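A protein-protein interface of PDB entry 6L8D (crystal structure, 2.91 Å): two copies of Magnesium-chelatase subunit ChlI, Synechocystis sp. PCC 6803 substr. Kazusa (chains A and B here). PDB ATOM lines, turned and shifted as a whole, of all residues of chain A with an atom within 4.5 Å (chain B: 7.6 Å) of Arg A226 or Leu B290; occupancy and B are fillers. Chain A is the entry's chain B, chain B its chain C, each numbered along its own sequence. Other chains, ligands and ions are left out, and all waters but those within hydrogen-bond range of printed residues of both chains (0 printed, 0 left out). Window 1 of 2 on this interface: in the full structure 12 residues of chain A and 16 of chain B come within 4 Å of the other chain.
The side-chain carboxylate (OD1) of Asp B293 is in salt-bridge range of the guanidinium group (NH2) of Arg A226, at 2.6 Å.
The guanidinium group of Arg A226 sits close to the backbone NH of Ala B283 (3.3 Å).
The guanidinium group of Arg A226 is in hydrogen-bond range of the backbone carbonyl oxygen of Gly B289 (3.0 Å).
The backbone carbonyl oxygen (O) of Cys B282 lies within hydrogen-bond range of the backbone NH (N) of Val B287.
The side-chain carboxylate of Asp B293 sits at hydrogen-bond distance from the side-chain hydroxyl of Ser B279, at 2.8 Å.
The side-chain sulfur of Cys B282 sits at hydrogen-bond distance from the side-chain carboxylate of Asp B293, at 3.2 Å.
O of Val A220 lies close to NH1 of Arg A226 (3.4 Å).
O of Val B278 is in hydrogen-bond range of SG of Cys B282.
Pro A223 touches Val B276 (CB to CG1, 3.8 Å).
Val B276 touches Glu A224.
OG of Ser B279 touches CB of Arg A226 (3.9 Å).
Cys B282 touches Arg A226 (CB to NH2, 3.7 Å).
Leu B290 touches Arg A226 (CD2 to NE, 3.3 Å).
Val A227 touches Arg B275.
CG2 of Val A227 touches CG2 of Val B276 (3.7 Å).
Ser B279 touches Val A227.
Ile A229 touches Leu B290 (CG2 to CD1, 3.7 Å).
CG1 of Val A230 touches CG1 of Ile B294 (3.8 Å).
Of chain B, only Ser B279, Cys B282, Ala B283, Gly B289, Leu B290 and Asp B293 come within 4 Å of Arg A226.
Printed residues of chain B within 4 Å of Glu A224: Val B276.
Printed residues of chain A within 4 Å of Val B276: Pro A223 (3.8 Å), Glu A224 (3.8 Å) and Val A227 (3.7 Å).
Of the printed residues of chain A, Cys B282 touches Arg A226.
Printed residues of chain B within 4 Å of Pro A223: Val B276 (3.8 Å), Ser B279 (3.8 Å) and Glu B280 (3.7 Å).
Of the printed residues of chain A, Ala B283 touches Arg A226.
Arg B291 touches none of the printed residues of chain A.
The nearest residue of chain B that does not touch Arg A226 is Val B287 (4.3 Å).
The nearest printed residue of chain A that does not touch Arg B275 is Pro A223 (5.9 Å).
Hydrophobic or aromatic side chains of chain A that line the printed part of chain B: Pro A223, Val A227, Ile A229 and Val A230.
Among the printed residues, 16 pairs touch across the chains.
No position is printed for both chains.
Of the 16 pairs that touch across the chains among the printed residues, none has its exchanged pair printed and touching as well.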
ATOM      1  N   VAL A 220      -8.638  -9.973 -22.270  1.00  0.00           N
ATOM      2  CA  VAL A 220      -8.857 -10.209 -20.848  1.00  0.00           C
ATOM      3  C   VAL A 220      -8.013  -9.263 -20.004  1.00  0.00           C
ATOM      4  O   VAL A 220      -6.829  -9.036 -20.280  1.00  0.00           O
ATOM      5  CB  VAL A 220      -8.556 -11.676 -20.510  1.00  0.00           C
ATOM      6  CG1 VAL A 220      -8.967 -11.984 -19.082  1.00  0.00           C
ATOM      7  CG2 VAL A 220      -9.276 -12.588 -21.486  1.00  0.00           C
ATOM      8  N   GLU A 222      -8.094  -9.534 -16.407  1.00  0.00           N
ATOM      9  CA  GLU A 222      -7.715 -10.154 -15.146  1.00  0.00           C
ATOM     10  C   GLU A 222      -6.311 -10.722 -15.295  1.00  0.00           C
ATOM     11  O   GLU A 222      -6.109 -11.637 -16.106  1.00  0.00           O
ATOM     12  CB  GLU A 222      -8.709 -11.248 -14.760  1.00  0.00           C
ATOM     13  N   PRO A 223      -5.321 -10.219 -14.550  1.00  0.00           N
ATOM     14  CA  PRO A 223      -3.934 -10.660 -14.795  1.00  0.00           C
ATOM     15  C   PRO A 223      -3.748 -12.162 -14.682  1.00  0.00           C
ATOM     16  O   PRO A 223      -3.177 -12.786 -15.589  1.00  0.00           O
ATOM     17  CB  PRO A 223      -3.142  -9.892 -13.730  1.00  0.00           C
ATOM     18  CG  PRO A 223      -3.977  -8.675 -13.446  1.00  0.00           C
ATOM     19  CD  PRO A 223      -5.397  -9.153 -13.535  1.00  0.00           C
ATOM     20  N   GLU A 224      -4.250 -12.768 -13.605  1.00  0.00           N
ATOM     21  CA  GLU A 224      -4.078 -14.202 -13.410  1.00  0.00           C
ATOM     22  C   GLU A 224      -4.806 -15.003 -14.479  1.00  0.00           C
ATOM     23  O   GLU A 224      -4.476 -16.175 -14.697  1.00  0.00           O
ATOM     24  CB  GLU A 224      -4.538 -14.613 -12.003  1.00  0.00           C
ATOM     25  CG  GLU A 224      -5.660 -13.763 -11.392  1.00  0.00           C
ATOM     26  CD  GLU A 224      -5.187 -12.406 -10.853  1.00  0.00           C
ATOM     27  OE1 GLU A 224      -5.867 -11.384 -11.132  1.00  0.00           O
ATOM     28  OE2 GLU A 224      -4.141 -12.363 -10.160  1.00  0.00           O
ATOM     29  N   LEU A 225      -5.784 -14.394 -15.155  1.00  0.00           N
ATOM     30  CA  LEU A 225      -6.430 -15.053 -16.283  1.00  0.00           C
ATOM     31  C   LEU A 225      -5.548 -15.022 -17.526  1.00  0.00           C
ATOM     32  O   LEU A 225      -5.440 -16.027 -18.238  1.00  0.00           O
ATOM     33  CB  LEU A 225      -7.771 -14.389 -16.581  1.00  0.00           C
ATOM     34  CG  LEU A 225      -9.028 -15.086 -16.066  1.00  0.00           C
ATOM     35  CD1 LEU A 225     -10.219 -14.523 -16.809  1.00  0.00           C
ATOM     36  CD2 LEU A 225      -8.936 -16.593 -16.240  1.00  0.00           C
ATOM     37  N   ARG A 226      -4.914 -13.874 -17.792  1.00  0.00           N
ATOM     38  CA  ARG A 226      -3.999 -13.761 -18.924  1.00  0.00           C
ATOM     39  C   ARG A 226      -2.873 -14.783 -18.830  1.00  0.00           C
ATOM     40  O   ARG A 226      -2.519 -15.423 -19.829  1.00  0.00           O
ATOM     41  CB  ARG A 226      -3.433 -12.343 -18.995  1.00  0.00           C
ATOM     42  CG  ARG A 226      -4.503 -11.273 -18.952  1.00  0.00           C
ATOM     43  CD  ARG A 226      -3.927  -9.876 -19.045  1.00  0.00           C
ATOM     44  NE  ARG A 226      -3.201  -9.683 -20.294  1.00  0.00           N
ATOM     45  CZ  ARG A 226      -3.150  -8.535 -20.958  1.00  0.00           C
ATOM     46  NH1 ARG A 226      -3.791  -7.477 -20.497  1.00  0.00           N
ATOM     47  NH2 ARG A 226      -2.465  -8.449 -22.087  1.00  0.00           N
ATOM     48  N   VAL A 227      -2.307 -14.964 -17.637  1.00  0.00           N
ATOM     49  CA  VAL A 227      -1.261 -15.968 -17.481  1.00  0.00           C
ATOM     50  C   VAL A 227      -1.807 -17.349 -17.825  1.00  0.00           C
ATOM     51  O   VAL A 227      -1.126 -18.162 -18.464  1.00  0.00           O
ATOM     52  CB  VAL A 227      -0.673 -15.918 -16.059  1.00  0.00           C
ATOM     53  CG1 VAL A 227       0.306 -17.059 -15.842  1.00  0.00           C
ATOM     54  CG2 VAL A 227       0.004 -14.575 -15.823  1.00  0.00           C
ATOM     55  N   LYS A 228      -3.054 -17.627 -17.423  1.00  0.00           N
ATOM     56  CA  LYS A 228      -3.644 -18.934 -17.697  1.00  0.00           C
ATOM     57  C   LYS A 228      -3.833 -19.163 -19.192  1.00  0.00           C
ATOM     58  O   LYS A 228      -3.556 -20.260 -19.691  1.00  0.00           O
ATOM     59  CB  LYS A 228      -4.981 -19.082 -16.978  1.00  0.00           C
ATOM     60  CG  LYS A 228      -5.687 -20.389 -17.325  1.00  0.00           C
ATOM     61  CD  LYS A 228      -7.084 -20.472 -16.741  1.00  0.00           C
ATOM     62  CE  LYS A 228      -7.662 -21.856 -16.971  1.00  0.00           C
ATOM     63  NZ  LYS A 228      -9.035 -21.989 -16.420  1.00  0.00           N
ATOM     64  N   ILE A 229      -4.302 -18.143 -19.923  1.00  0.00           N
ATOM     65  CA  ILE A 229      -4.497 -18.303 -21.362  1.00  0.00           C
ATOM     66  C   ILE A 229      -3.183 -18.673 -22.028  1.00  0.00           C
ATOM     67  O   ILE A 229      -3.110 -19.631 -22.807  1.00  0.00           O
ATOM     68  CB  ILE A 229      -5.092 -17.032 -21.989  1.00  0.00           C
ATOM     69  CG1 ILE A 229      -6.381 -16.619 -21.292  1.00  0.00           C
ATOM     70  CG2 ILE A 229      -5.345 -17.247 -23.472  1.00  0.00           C
ATOM     71  CD1 ILE A 229      -7.007 -15.375 -21.880  1.00  0.00           C
ATOM     72  N   VAL A 230      -2.120 -17.918 -21.724  1.00  0.00           N
ATOM     73  CA  VAL A 230      -0.818 -18.186 -22.331  1.00  0.00           C
ATOM     74  C   VAL A 230      -0.324 -19.569 -21.931  1.00  0.00           C
ATOM     75  O   VAL A 230       0.093 -20.369 -22.777  1.00  0.00           O
ATOM     76  CB  VAL A 230       0.197 -17.099 -21.936  1.00  0.00           C
ATOM     77  CG1 VAL A 230       1.562 -17.410 -22.535  1.00  0.00           C
ATOM     78  CG2 VAL A 230      -0.294 -15.727 -22.356  1.00  0.00           C
ATOM     79  N   ARG A 233      -1.927 -22.136 -23.861  1.00  0.00           N
ATOM     80  CA  ARG A 233      -1.516 -22.215 -25.258  1.00  0.00           C
ATOM     81  C   ARG A 233      -0.265 -23.075 -25.409  1.00  0.00           C
ATOM     82  O   ARG A 233      -0.214 -23.971 -26.260  1.00  0.00           O
ATOM     83  CB  ARG A 233      -1.281 -20.813 -25.822  1.00  0.00           C
ATOM     84  CG  ARG A 233      -2.544 -20.057 -26.199  1.00  0.00           C
ATOM     85  CD  ARG A 233      -2.193 -18.735 -26.853  1.00  0.00           C
ATOM     86  NE  ARG A 233      -3.308 -17.792 -26.831  1.00  0.00           N
ATOM     87  CZ  ARG A 233      -3.213 -16.510 -27.181  1.00  0.00           C
ATOM     88  NH1 ARG A 233      -2.045 -16.010 -27.580  1.00  0.00           N
ATOM     89  NH2 ARG A 233      -4.285 -15.727 -27.127  1.00  0.00           N
ATOM     90  N   ARG B 275       5.271 -13.404 -13.121  1.00  0.00           N
ATOM     91  CA  ARG B 275       4.566 -13.577 -14.388  1.00  0.00           C
ATOM     92  C   ARG B 275       3.196 -12.910 -14.369  1.00  0.00           C
ATOM     93  O   ARG B 275       2.750 -12.382 -15.394  1.00  0.00           O
ATOM     94  CB  ARG B 275       4.451 -15.064 -14.715  1.00  0.00           C
ATOM     95  CG  ARG B 275       3.964 -15.338 -16.126  1.00  0.00           C
ATOM     96  CD  ARG B 275       4.011 -16.823 -16.446  1.00  0.00           C
ATOM     97  NE  ARG B 275       4.741 -17.569 -15.426  1.00  0.00           N
ATOM     98  CZ  ARG B 275       4.413 -18.795 -15.031  1.00  0.00           C
ATOM     99  NH1 ARG B 275       3.362 -19.404 -15.575  1.00  0.00           N
ATOM    100  NH2 ARG B 275       5.124 -19.410 -14.089  1.00  0.00           N
ATOM    101  N   VAL B 276       2.521 -12.914 -13.220  1.00  0.00           N
ATOM    102  CA  VAL B 276       1.229 -12.249 -13.121  1.00  0.00           C
ATOM    103  C   VAL B 276       1.416 -10.741 -13.105  1.00  0.00           C
ATOM    104  O   VAL B 276       0.657  -9.998 -13.741  1.00  0.00           O
ATOM    105  CB  VAL B 276       0.462 -12.736 -11.882  1.00  0.00           C
ATOM    106  CG1 VAL B 276      -0.684 -11.786 -11.567  1.00  0.00           C
ATOM    107  CG2 VAL B 276      -0.050 -14.154 -12.099  1.00  0.00           C
ATOM    108  N   VAL B 278       3.693  -9.111 -14.527  1.00  0.00           N
ATOM    109  CA  VAL B 278       3.965  -8.715 -15.905  1.00  0.00           C
ATOM    110  C   VAL B 278       2.660  -8.544 -16.665  1.00  0.00           C
ATOM    111  O   VAL B 278       2.468  -7.566 -17.396  1.00  0.00           O
ATOM    112  CB  VAL B 278       4.888  -9.739 -16.593  1.00  0.00           C
ATOM    113  CG1 VAL B 278       4.946  -9.485 -18.087  1.00  0.00           C
ATOM    114  CG2 VAL B 278       6.280  -9.688 -15.996  1.00  0.00           C
ATOM    115  N   SER B 279       1.740  -9.498 -16.507  1.00  0.00           N
ATOM    116  CA  SER B 279       0.454  -9.383 -17.185  1.00  0.00           C
ATOM    117  C   SER B 279      -0.364  -8.216 -16.649  1.00  0.00           C
ATOM    118  O   SER B 279      -1.087  -7.568 -17.413  1.00  0.00           O
ATOM    119  CB  SER B 279      -0.323 -10.691 -17.068  1.00  0.00           C
ATOM    120  OG  SER B 279       0.240 -11.675 -17.918  1.00  0.00           O
ATOM    121  N   GLU B 280      -0.265  -7.928 -15.349  1.00  0.00           N
ATOM    122  CA  GLU B 280      -0.957  -6.763 -14.809  1.00  0.00           C
ATOM    123  C   GLU B 280      -0.440  -5.472 -15.437  1.00  0.00           C
ATOM    124  O   GLU B 280      -1.215  -4.534 -15.668  1.00  0.00           O
ATOM    125  CB  GLU B 280      -0.836  -6.729 -13.285  1.00  0.00           C
ATOM    126  CG  GLU B 280      -1.425  -5.474 -12.657  1.00  0.00           C
ATOM    127  CD  GLU B 280      -1.715  -5.638 -11.175  1.00  0.00           C
ATOM    128  OE1 GLU B 280      -1.209  -6.606 -10.562  1.00  0.00           O
ATOM    129  OE2 GLU B 280      -2.478  -4.811 -10.633  1.00  0.00           O
ATOM    130  N   VAL B 281       0.868  -5.398 -15.715  1.00  0.00           N
ATOM    131  CA  VAL B 281       1.422  -4.223 -16.387  1.00  0.00           C
ATOM    132  C   VAL B 281       0.841  -4.087 -17.791  1.00  0.00           C
ATOM    133  O   VAL B 281       0.478  -2.988 -18.229  1.00  0.00           O
ATOM    134  CB  VAL B 281       2.959  -4.301 -16.437  1.00  0.00           C
ATOM    135  CG1 VAL B 281       3.515  -3.162 -17.286  1.00  0.00           C
ATOM    136  CG2 VAL B 281       3.546  -4.281 -15.046  1.00  0.00           C
ATOM    137  N   CYS B 282       0.742  -5.207 -18.516  1.00  0.00           N
ATOM    138  CA  CYS B 282       0.177  -5.178 -19.860  1.00  0.00           C
ATOM    139  C   CYS B 282      -1.275  -4.717 -19.843  1.00  0.00           C
ATOM    140  O   CYS B 282      -1.703  -3.958 -20.721  1.00  0.00           O
ATOM    141  CB  CYS B 282       0.280  -6.559 -20.507  1.00  0.00           C
ATOM    142  SG  CYS B 282       1.949  -7.161 -20.821  1.00  0.00           S
ATOM    143  N   ALA B 283      -2.047  -5.157 -18.845  1.00  0.00           N
ATOM    144  CA  ALA B 283      -3.455  -4.783 -18.781  1.00  0.00           C
ATOM    145  C   ALA B 283      -3.609  -3.294 -18.523  1.00  0.00           C
ATOM    146  O   ALA B 283      -4.402  -2.617 -19.187  1.00  0.00           O
ATOM    147  CB  ALA B 283      -4.163  -5.592 -17.699  1.00  0.00           C
ATOM    148  N   GLU B 284      -2.853  -2.760 -17.565  1.00  0.00           N
ATOM    149  CA  GLU B 284      -2.950  -1.338 -17.276  1.00  0.00           C
ATOM    150  C   GLU B 284      -2.438  -0.485 -18.432  1.00  0.00           C
ATOM    151  O   GLU B 284      -2.754   0.707 -18.490  1.00  0.00           O
ATOM    152  CB  GLU B 284      -2.204  -1.025 -15.982  1.00  0.00           C
ATOM    153  CG  GLU B 284      -2.560   0.314 -15.365  1.00  0.00           C
ATOM    154  CD  GLU B 284      -2.226   0.370 -13.888  1.00  0.00           C
ATOM    155  OE1 GLU B 284      -2.530  -0.616 -13.184  1.00  0.00           O
ATOM    156  OE2 GLU B 284      -1.661   1.388 -13.431  1.00  0.00           O
ATOM    157  N   LEU B 285      -1.662  -1.068 -19.347  1.00  0.00           N
ATOM    158  CA  LEU B 285      -1.232  -0.404 -20.575  1.00  0.00           C
ATOM    159  C   LEU B 285      -2.224  -0.549 -21.721  1.00  0.00           C
ATOM    160  O   LEU B 285      -1.992   0.025 -22.788  1.00  0.00           O
ATOM    161  CB  LEU B 285       0.127  -0.950 -21.028  1.00  0.00           C
ATOM    162  CG  LEU B 285       1.384  -0.211 -20.577  1.00  0.00           C
ATOM    163  CD1 LEU B 285       1.259   0.247 -19.156  1.00  0.00           C
ATOM    164  CD2 LEU B 285       2.612  -1.090 -20.753  1.00  0.00           C
ATOM    165  N   ASP B 286      -3.306  -1.306 -21.534  1.00  0.00           N
ATOM    166  CA  ASP B 286      -4.302  -1.539 -22.582  1.00  0.00           C
ATOM    167  C   ASP B 286      -3.662  -2.134 -23.835  1.00  0.00           C
ATOM    168  O   ASP B 286      -3.898  -1.687 -24.957  1.00  0.00           O
ATOM    169  CB  ASP B 286      -5.059  -0.256 -22.921  1.00  0.00           C
ATOM    170  CG  ASP B 286      -6.331  -0.527 -23.686  1.00  0.00           C
ATOM    171  OD1 ASP B 286      -6.752  -1.704 -23.725  1.00  0.00           O
ATOM    172  OD2 ASP B 286      -6.887   0.425 -24.278  1.00  0.00           O
ATOM    173  N   VAL B 287      -2.851  -3.170 -23.629  1.00  0.00           N
ATOM    174  CA  VAL B 287      -2.162  -3.825 -24.729  1.00  0.00           C
ATOM    175  C   VAL B 287      -3.160  -4.609 -25.574  1.00  0.00           C
ATOM    176  O   VAL B 287      -4.106  -5.215 -25.053  1.00  0.00           O
ATOM    177  CB  VAL B 287      -1.045  -4.717 -24.159  1.00  0.00           C
ATOM    178  CG1 VAL B 287      -0.729  -5.898 -25.078  1.00  0.00           C
ATOM    179  CG2 VAL B 287       0.193  -3.880 -23.885  1.00  0.00           C
ATOM    180  N   ASP B 288      -2.958  -4.588 -26.891  1.00  0.00           N
ATOM    181  CA  ASP B 288      -3.818  -5.278 -27.854  1.00  0.00           C
ATOM    182  C   ASP B 288      -3.423  -6.751 -27.900  1.00  0.00           C
ATOM    183  O   ASP B 288      -2.536  -7.155 -28.651  1.00  0.00           O
ATOM    184  CB  ASP B 288      -3.694  -4.625 -29.226  1.00  0.00           C
ATOM    185  CG  ASP B 288      -4.814  -5.018 -30.176  1.00  0.00           C
ATOM    186  OD1 ASP B 288      -5.255  -6.185 -30.162  1.00  0.00           O
ATOM    187  OD2 ASP B 288      -5.244  -4.145 -30.958  1.00  0.00           O
ATOM    188  N   GLY B 289      -4.099  -7.572 -27.117  1.00  0.00           N
ATOM    189  CA  GLY B 289      -3.836  -8.993 -27.147  1.00  0.00           C
ATOM    190  C   GLY B 289      -2.896  -9.411 -26.038  1.00  0.00           C
ATOM    191  O   GLY B 289      -2.628  -8.671 -25.089  1.00  0.00           O
ATOM    192  N   LEU B 290      -2.385 -10.633 -26.170  1.00  0.00           N
ATOM    193  CA  LEU B 290      -1.458 -11.192 -25.196  1.00  0.00           C
ATOM    194  C   LEU B 290      -0.032 -11.259 -25.730  1.00  0.00           C
ATOM    195  O   LEU B 290       0.847 -11.819 -25.065  1.00  0.00           O
ATOM    196  CB  LEU B 290      -1.924 -12.581 -24.765  1.00  0.00           C
ATOM    197  CG  LEU B 290      -3.267 -12.634 -24.042  1.00  0.00           C
ATOM    198  CD1 LEU B 290      -3.535 -14.042 -23.555  1.00  0.00           C
ATOM    199  CD2 LEU B 290      -3.315 -11.642 -22.897  1.00  0.00           C
ATOM    200  N   ARG B 291       0.216 -10.703 -26.918  1.00  0.00           N
ATOM    201  CA  ARG B 291       1.544 -10.778 -27.518  1.00  0.00           C
ATOM    202  C   ARG B 291       2.574 -10.045 -26.673  1.00  0.00           C
ATOM    203  O   ARG B 291       3.722 -10.488 -26.561  1.00  0.00           O
ATOM    204  CB  ARG B 291       1.502 -10.204 -28.932  1.00  0.00           C
ATOM    205  CG  ARG B 291       2.810 -10.269 -29.684  1.00  0.00           C
ATOM    206  CD  ARG B 291       3.239 -11.698 -29.920  1.00  0.00           C
ATOM    207  NE  ARG B 291       4.636 -11.782 -30.336  1.00  0.00           N
ATOM    208  CZ  ARG B 291       5.349 -12.902 -30.319  1.00  0.00           C
ATOM    209  NH1 ARG B 291       4.796 -14.033 -29.897  1.00  0.00           N
ATOM    210  NH2 ARG B 291       6.615 -12.889 -30.716  1.00  0.00           N
ATOM    211  N   GLY B 292       2.189  -8.910 -26.087  1.00  0.00           N
ATOM    212  CA  GLY B 292       3.095  -8.202 -25.195  1.00  0.00           C
ATOM    213  C   GLY B 292       3.429  -8.992 -23.944  1.00  0.00           C
ATOM    214  O   GLY B 292       4.574  -8.993 -23.485  1.00  0.00           O
ATOM    215  N   ASP B 293       2.437  -9.690 -23.385  1.00  0.00           N
ATOM    216  CA  ASP B 293       2.692 -10.540 -22.227  1.00  0.00           C
ATOM    217  C   ASP B 293       3.716 -11.621 -22.552  1.00  0.00           C
ATOM    218  O   ASP B 293       4.577 -11.938 -21.726  1.00  0.00           O
ATOM    219  CB  ASP B 293       1.389 -11.171 -21.739  1.00  0.00           C
ATOM    220  CG  ASP B 293       0.335 -10.134 -21.369  1.00  0.00           C
ATOM    221  OD1 ASP B 293       0.000  -9.295 -22.230  1.00  0.00           O
ATOM    222  OD2 ASP B 293      -0.171 -10.170 -20.225  1.00  0.00           O
ATOM    223  N   ILE B 294       3.650 -12.185 -23.759  1.00  0.00           N
ATOM    224  CA  ILE B 294       4.524 -13.303 -24.099  1.00  0.00           C
ATOM    225  C   ILE B 294       5.956 -12.822 -24.321  1.00  0.00           C
ATOM    226  O   ILE B 294       6.904 -13.413 -23.793  1.00  0.00           O
ATOM    227  CB  ILE B 294       3.985 -14.049 -25.331  1.00  0.00           C
ATOM    228  CG1 ILE B 294       2.668 -14.743 -24.998  1.00  0.00           C
ATOM    229  CG2 ILE B 294       4.995 -15.056 -25.831  1.00  0.00           C
ATOM    230  CD1 ILE B 294       1.923 -15.223 -26.215  1.00  0.00           C
ATOM    231  N   VAL B 295       6.140 -11.725 -25.071  1.00  0.00           N
ATOM    232  CA  VAL B 295       7.507 -11.304 -25.385  1.00  0.00           C
ATOM    233  C   VAL B 295       8.230 -10.838 -24.126  1.00  0.00           C
ATOM    234  O   VAL B 295       9.375 -11.233 -23.886  1.00  0.00           O
ATOM    235  CB  VAL B 295       7.540 -10.236 -26.497  1.00  0.00           C
ATOM    236  CG1 VAL B 295       6.888 -10.773 -27.760  1.00  0.00           C
ATOM    237  CG2 VAL B 295       6.888  -8.948 -26.055  1.00  0.00           C
ATOM    238  N   THR B 296       7.563 -10.049 -23.272  1.00  0.00           N
ATOM    239  CA  THR B 296       8.188  -9.624 -22.023  1.00  0.00           C
ATOM    240  C   THR B 296       8.664 -10.825 -21.226  1.00  0.00           C
ATOM    241  O   THR B 296       9.739 -10.797 -20.616  1.00  0.00           O
ATOM    242  CB  THR B 296       7.217  -8.792 -21.190  1.00  0.00           C
ATOM    243  OG1 THR B 296       6.754  -7.679 -21.960  1.00  0.00           O
ATOM    244  CG2 THR B 296       7.891  -8.275 -19.946  1.00  0.00           C
ATOM    245  N   ARG B 328       3.423  -1.019 -27.978  1.00  0.00           N
ATOM    246  CA  ARG B 328       2.145  -1.698 -27.851  1.00  0.00           C
ATOM    247  C   ARG B 328       1.153  -0.880 -27.036  1.00  0.00           C
ATOM    248  O   ARG B 328       0.110  -1.401 -26.627  1.00  0.00           O
ATOM    249  CB  ARG B 328       2.360  -3.086 -27.243  1.00  0.00           C
ATOM    250  CG  ARG B 328       3.188  -3.996 -28.146  1.00  0.00           C
ATOM    251  CD  ARG B 328       3.333  -5.397 -27.583  1.00  0.00           C
ATOM    252  NE  ARG B 328       3.564  -6.367 -28.649  1.00  0.00           N
ATOM    253  CZ  ARG B 328       4.758  -6.824 -29.004  1.00  0.00           C
ATOM    254  NH1 ARG B 328       5.843  -6.413 -28.367  1.00  0.00           N
ATOM    255  NH2 ARG B 328       4.869  -7.700 -29.992  1.00  0.00           N
